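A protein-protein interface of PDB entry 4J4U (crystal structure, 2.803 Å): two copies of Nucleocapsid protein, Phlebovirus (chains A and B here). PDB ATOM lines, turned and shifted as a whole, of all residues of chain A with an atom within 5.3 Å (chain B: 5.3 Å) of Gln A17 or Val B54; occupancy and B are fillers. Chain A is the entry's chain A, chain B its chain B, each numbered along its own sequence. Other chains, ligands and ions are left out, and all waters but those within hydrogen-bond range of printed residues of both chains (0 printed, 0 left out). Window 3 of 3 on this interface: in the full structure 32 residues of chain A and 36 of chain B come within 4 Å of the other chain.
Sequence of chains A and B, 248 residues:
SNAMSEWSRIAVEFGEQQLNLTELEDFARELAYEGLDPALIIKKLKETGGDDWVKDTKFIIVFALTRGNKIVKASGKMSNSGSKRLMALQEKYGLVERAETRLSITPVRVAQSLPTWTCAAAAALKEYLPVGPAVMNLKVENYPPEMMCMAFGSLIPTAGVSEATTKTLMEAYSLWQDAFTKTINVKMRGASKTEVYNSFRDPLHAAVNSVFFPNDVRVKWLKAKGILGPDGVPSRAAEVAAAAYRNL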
ATOM      1  N   GLU A  13      24.701  14.735 -11.708  1.00  0.00           N
ATOM      2  CA  GLU A  13      24.839  16.191 -11.468  1.00  0.00           C
ATOM      3  C   GLU A  13      24.909  17.052 -12.756  1.00  0.00           C
ATOM      4  O   GLU A  13      24.287  18.106 -12.826  1.00  0.00           O
ATOM      5  CB  GLU A  13      26.029  16.521 -10.535  1.00  0.00           C
ATOM      6  CG  GLU A  13      25.902  16.062  -9.065  1.00  0.00           C
ATOM      7  CD  GLU A  13      24.795  16.773  -8.270  1.00  0.00           C
ATOM      8  OE1 GLU A  13      24.745  18.029  -8.276  1.00  0.00           O
ATOM      9  OE2 GLU A  13      23.976  16.065  -7.628  1.00  0.00           O
ATOM     10  N   PHE A  14      25.663  16.608 -13.761  1.00  0.00           N
ATOM     11  CA  PHE A  14      25.680  17.262 -15.078  1.00  0.00           C
ATOM     12  C   PHE A  14      24.260  17.404 -15.650  1.00  0.00           C
ATOM     13  O   PHE A  14      23.943  18.371 -16.354  1.00  0.00           O
ATOM     14  CB  PHE A  14      26.564  16.465 -16.061  1.00  0.00           C
ATOM     15  CG  PHE A  14      27.253  17.319 -17.114  1.00  0.00           C
ATOM     16  CD1 PHE A  14      26.587  17.715 -18.259  1.00  0.00           C
ATOM     17  CD2 PHE A  14      28.573  17.711 -16.954  1.00  0.00           C
ATOM     18  CE1 PHE A  14      27.218  18.499 -19.205  1.00  0.00           C
ATOM     19  CE2 PHE A  14      29.209  18.483 -17.906  1.00  0.00           C
ATOM     20  CZ  PHE A  14      28.530  18.880 -19.026  1.00  0.00           C
ATOM     21  N   GLY A  15      23.419  16.414 -15.353  1.00  0.00           N
ATOM     22  CA  GLY A  15      22.026  16.431 -15.755  1.00  0.00           C
ATOM     23  C   GLY A  15      21.198  17.405 -14.936  1.00  0.00           C
ATOM     24  O   GLY A  15      20.258  17.995 -15.448  1.00  0.00           O
ATOM     25  N   GLU A  16      21.551  17.571 -13.660  1.00  0.00           N
ATOM     26  CA  GLU A  16      20.848  18.482 -12.749  1.00  0.00           C
ATOM     27  C   GLU A  16      20.957  19.957 -13.182  1.00  0.00           C
ATOM     28  O   GLU A  16      20.131  20.790 -12.792  1.00  0.00           O
ATOM     29  CB  GLU A  16      21.363  18.322 -11.308  1.00  0.00           C
ATOM     30  CG  GLU A  16      20.908  17.063 -10.549  1.00  0.00           C
ATOM     31  CD  GLU A  16      21.488  16.993  -9.107  1.00  0.00           C
ATOM     32  OE1 GLU A  16      22.053  18.007  -8.621  1.00  0.00           O
ATOM     33  OE2 GLU A  16      21.382  15.917  -8.465  1.00  0.00           O
ATOM     34  N   GLN A  17      21.966  20.275 -13.990  1.00  0.00           N
ATOM     35  CA  GLN A  17      22.222  21.663 -14.394  1.00  0.00           C
ATOM     36  C   GLN A  17      21.038  22.321 -15.101  1.00  0.00           C
ATOM     37  O   GLN A  17      20.095  21.652 -15.510  1.00  0.00           O
ATOM     38  CB  GLN A  17      23.484  21.766 -15.254  1.00  0.00           C
ATOM     39  CG  GLN A  17      24.792  21.688 -14.463  1.00  0.00           C
ATOM     40  CD  GLN A  17      26.007  21.946 -15.330  1.00  0.00           C
ATOM     41  OE1 GLN A  17      26.091  21.461 -16.454  1.00  0.00           O
ATOM     42  NE2 GLN A  17      26.956  22.717 -14.810  1.00  0.00           N
ATOM     43  N   GLN A  18      21.083  23.638 -15.229  1.00  0.00           N
ATOM     44  CA  GLN A  18      20.005  24.347 -15.897  1.00  0.00           C
ATOM     45  C   GLN A  18      20.520  24.896 -17.220  1.00  0.00           C
ATOM     46  O   GLN A  18      21.606  25.439 -17.299  1.00  0.00           O
ATOM     47  CB  GLN A  18      19.427  25.461 -15.010  1.00  0.00           C
ATOM     48  CG  GLN A  18      19.141  25.057 -13.538  1.00  0.00           C
ATOM     49  CD  GLN A  18      17.720  24.527 -13.288  1.00  0.00           C
ATOM     50  OE1 GLN A  18      16.844  24.594 -14.159  1.00  0.00           O
ATOM     51  NE2 GLN A  18      17.494  24.003 -12.083  1.00  0.00           N
ATOM     52  N   LEU A  19      19.723  24.734 -18.258  1.00  0.00           N
ATOM     53  CA  LEU A  19      20.117  25.117 -19.596  1.00  0.00           C
ATOM     54  C   LEU A  19      20.120  26.629 -19.787  1.00  0.00           C
ATOM     55  O   LEU A  19      19.187  27.313 -19.392  1.00  0.00           O
ATOM     56  CB  LEU A  19      19.160  24.481 -20.607  1.00  0.00           C
ATOM     57  CG  LEU A  19      19.376  23.040 -21.076  1.00  0.00           C
ATOM     58  CD1 LEU A  19      19.975  22.156 -19.998  1.00  0.00           C
ATOM     59  CD2 LEU A  19      18.055  22.443 -21.605  1.00  0.00           C
ATOM     60  N   ASP B  51      38.444  22.579 -16.048  1.00  0.00           N
ATOM     61  CA  ASP B  51      37.134  23.137 -15.816  1.00  0.00           C
ATOM     62  C   ASP B  51      36.475  23.577 -17.121  1.00  0.00           C
ATOM     63  O   ASP B  51      35.261  23.683 -17.163  1.00  0.00           O
ATOM     64  CB  ASP B  51      37.205  24.276 -14.790  1.00  0.00           C
ATOM     65  CG  ASP B  51      37.579  23.787 -13.383  1.00  0.00           C
ATOM     66  OD1 ASP B  51      37.866  22.576 -13.216  1.00  0.00           O
ATOM     67  OD2 ASP B  51      37.563  24.622 -12.444  1.00  0.00           O
ATOM     68  N   ASP B  52      37.243  23.799 -18.197  1.00  0.00           N
ATOM     69  CA  ASP B  52      36.602  24.129 -19.486  1.00  0.00           C
ATOM     70  C   ASP B  52      35.816  22.908 -19.979  1.00  0.00           C
ATOM     71  O   ASP B  52      35.026  23.016 -20.912  1.00  0.00           O
ATOM     72  CB  ASP B  52      37.573  24.650 -20.593  1.00  0.00           C
ATOM     73  CG  ASP B  52      36.818  25.268 -21.834  1.00  0.00           C
ATOM     74  OD1 ASP B  52      35.727  25.805 -21.620  1.00  0.00           O
ATOM     75  OD2 ASP B  52      37.274  25.224 -23.009  1.00  0.00           O
ATOM     76  N   TRP B  53      36.020  21.754 -19.342  1.00  0.00           N
ATOM     77  CA  TRP B  53      35.372  20.519 -19.796  1.00  0.00           C
ATOM     78  C   TRP B  53      33.846  20.568 -19.784  1.00  0.00           C
ATOM     79  O   TRP B  53      33.206  20.101 -20.726  1.00  0.00           O
ATOM     80  CB  TRP B  53      35.898  19.286 -19.051  1.00  0.00           C
ATOM     81  CG  TRP B  53      35.139  18.876 -17.823  1.00  0.00           C
ATOM     82  CD1 TRP B  53      35.368  19.295 -16.550  1.00  0.00           C
ATOM     83  CD2 TRP B  53      34.059  17.927 -17.739  1.00  0.00           C
ATOM     84  NE1 TRP B  53      34.500  18.685 -15.673  1.00  0.00           N
ATOM     85  CE2 TRP B  53      33.687  17.839 -16.375  1.00  0.00           C
ATOM     86  CE3 TRP B  53      33.370  17.150 -18.679  1.00  0.00           C
ATOM     87  CZ2 TRP B  53      32.660  17.015 -15.928  1.00  0.00           C
ATOM     88  CZ3 TRP B  53      32.335  16.321 -18.231  1.00  0.00           C
ATOM     89  CH2 TRP B  53      31.992  16.263 -16.866  1.00  0.00           C
ATOM     90  N   VAL B  54      33.271  21.160 -18.743  1.00  0.00           N
ATOM     91  CA  VAL B  54      31.816  21.270 -18.658  1.00  0.00           C
ATOM     92  C   VAL B  54      31.189  22.066 -19.811  1.00  0.00           C
ATOM     93  O   VAL B  54      30.201  21.623 -20.400  1.00  0.00           O
ATOM     94  CB  VAL B  54      31.356  21.783 -17.289  1.00  0.00           C
ATOM     95  CG1 VAL B  54      29.959  22.337 -17.366  1.00  0.00           C
ATOM     96  CG2 VAL B  54      31.418  20.651 -16.282  1.00  0.00           C
ATOM     97  N   LYS B  55      31.769  23.210 -20.164  1.00  0.00           N
ATOM     98  CA  LYS B  55      31.287  23.940 -21.332  1.00  0.00           C
ATOM     99  C   LYS B  55      31.672  23.264 -22.645  1.00  0.00           C
ATOM    100  O   LYS B  55      30.883  23.227 -23.585  1.00  0.00           O
ATOM    101  CB  LYS B  55      31.767  25.388 -21.343  1.00  0.00           C
ATOM    102  CG  LYS B  55      31.015  26.313 -20.370  1.00  0.00           C
ATOM    103  CD  LYS B  55      29.499  25.988 -20.263  1.00  0.00           C
ATOM    104  CE  LYS B  55      28.607  26.911 -21.111  1.00  0.00           C
ATOM    105  NZ  LYS B  55      27.207  26.972 -20.565  1.00  0.00           N
ATOM    106  N   ASP B  56      32.882  22.719 -22.710  1.00  0.00           N
ATOM    107  CA  ASP B  56      33.361  22.093 -23.936  1.00  0.00           C
ATOM    108  C   ASP B  56      32.478  20.933 -24.281  1.00  0.00           C
ATOM    109  O   ASP B  56      32.118  20.746 -25.441  1.00  0.00           O
ATOM    110  CB  ASP B  56      34.795  21.599 -23.775  1.00  0.00           C
ATOM    111  CG  ASP B  56      35.784  22.713 -23.675  1.00  0.00           C
ATOM    112  OD1 ASP B  56      35.384  23.893 -23.784  1.00  0.00           O
ATOM    113  OD2 ASP B  56      36.965  22.401 -23.490  1.00  0.00           O
ATOM    114  N   THR B  57      32.128  20.157 -23.261  1.00  0.00           N
ATOM    115  CA  THR B  57      31.198  19.048 -23.437  1.00  0.00           C
ATOM    116  C   THR B  57      29.831  19.466 -24.019  1.00  0.00           C
ATOM    117  O   THR B  57      29.393  18.893 -25.022  1.00  0.00           O
ATOM    118  CB  THR B  57      30.982  18.305 -22.135  1.00  0.00           C
ATOM    119  OG1 THR B  57      32.196  17.641 -21.786  1.00  0.00           O
ATOM    120  CG2 THR B  57      29.829  17.277 -22.266  1.00  0.00           C
ATOM    121  N   LYS B  58      29.175  20.451 -23.395  1.00  0.00           N
ATOM    122  CA  LYS B  58      27.896  20.966 -23.875  1.00  0.00           C
ATOM    123  C   LYS B  58      27.982  21.306 -25.349  1.00  0.00           C
ATOM    124  O   LYS B  58      27.034  21.064 -26.110  1.00  0.00           O
ATOM    125  CB  LYS B  58      27.445  22.201 -23.084  1.00  0.00           C
ATOM    126  CG  LYS B  58      27.079  21.875 -21.638  1.00  0.00           C
ATOM    127  CD  LYS B  58      26.876  23.076 -20.718  1.00  0.00           C
ATOM    128  CE  LYS B  58      26.528  22.553 -19.340  1.00  0.00           C
ATOM    129  NZ  LYS B  58      26.573  23.551 -18.238  1.00  0.00           N
ATOM    130  N   TRP B 117      21.273  15.596 -19.659  1.00  0.00           N
ATOM    131  CA  TRP B 117      21.552  16.910 -20.211  1.00  0.00           C
ATOM    132  C   TRP B 117      21.191  16.915 -21.703  1.00  0.00           C
ATOM    133  O   TRP B 117      20.444  17.779 -22.179  1.00  0.00           O
ATOM    134  CB  TRP B 117      23.019  17.340 -19.965  1.00  0.00           C
ATOM    135  CG  TRP B 117      23.218  18.785 -20.264  1.00  0.00           C
ATOM    136  CD1 TRP B 117      23.047  19.833 -19.409  1.00  0.00           C
ATOM    137  CD2 TRP B 117      23.561  19.354 -21.531  1.00  0.00           C
ATOM    138  NE1 TRP B 117      23.276  21.018 -20.061  1.00  0.00           N
ATOM    139  CE2 TRP B 117      23.588  20.753 -21.366  1.00  0.00           C
ATOM    140  CE3 TRP B 117      23.864  18.817 -22.784  1.00  0.00           C
ATOM    141  CZ2 TRP B 117      23.891  21.620 -22.407  1.00  0.00           C
ATOM    142  CZ3 TRP B 117      24.173  19.686 -23.815  1.00  0.00           C
ATOM    143  CH2 TRP B 117      24.182  21.071 -23.621  1.00  0.00           C
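Among the printed residues, pairs that only touch across the chains: Leu A19 with Trp B117, Phe A14 with Val B54, Phe A14 with Trp B117, Phe A14 with Trp B53, Phe A14 with Thr B57 and Gln A17 with Val B54.
No position is printed for both chains.
Of the 7 pairs that touch across the chains among the printed residues, none has its exchanged pair printed and touching as well.
OE1 of Gln A17 is in hydrogen-bond range of NZ of Lys B58, 2.8 Å away.
Printed residues of chain A within 4 Å of Trp B53: Phe A14.
Of the printed residues of chain A, Trp B117 touches Phe A14 and Leu A19.
Of the printed residues of chain B, Phe A14 touches Trp B53 (3.7 Å), Val B54 (3.5 Å), Thr B57 (3.8 Å) and Trp B117 (3.5 Å).
Gly A15 touches none of the printed residues of chain B.
Asp B52 touches none of the printed residues of chain A.
OG1 of Thr B57 lies within hydrogen-bond range of O of Trp B53, 2.9 Å away.
Of the 9 printed residues of chain B, 5 touch a printed residue of chain A.
Hydrophobic or aromatic side chains of chain B within 4 Å of the printed part of chain A: Trp B53, Val B54 and Trp B117.
Printed residues of chain A that touch a printed residue of chain B: Phe A14, Gln A17 and Leu A19.
Among the printed residues, no Asp or Glu carboxylate lies within 4 Å of a Lys or Arg side-chain nitrogen of the other chain.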
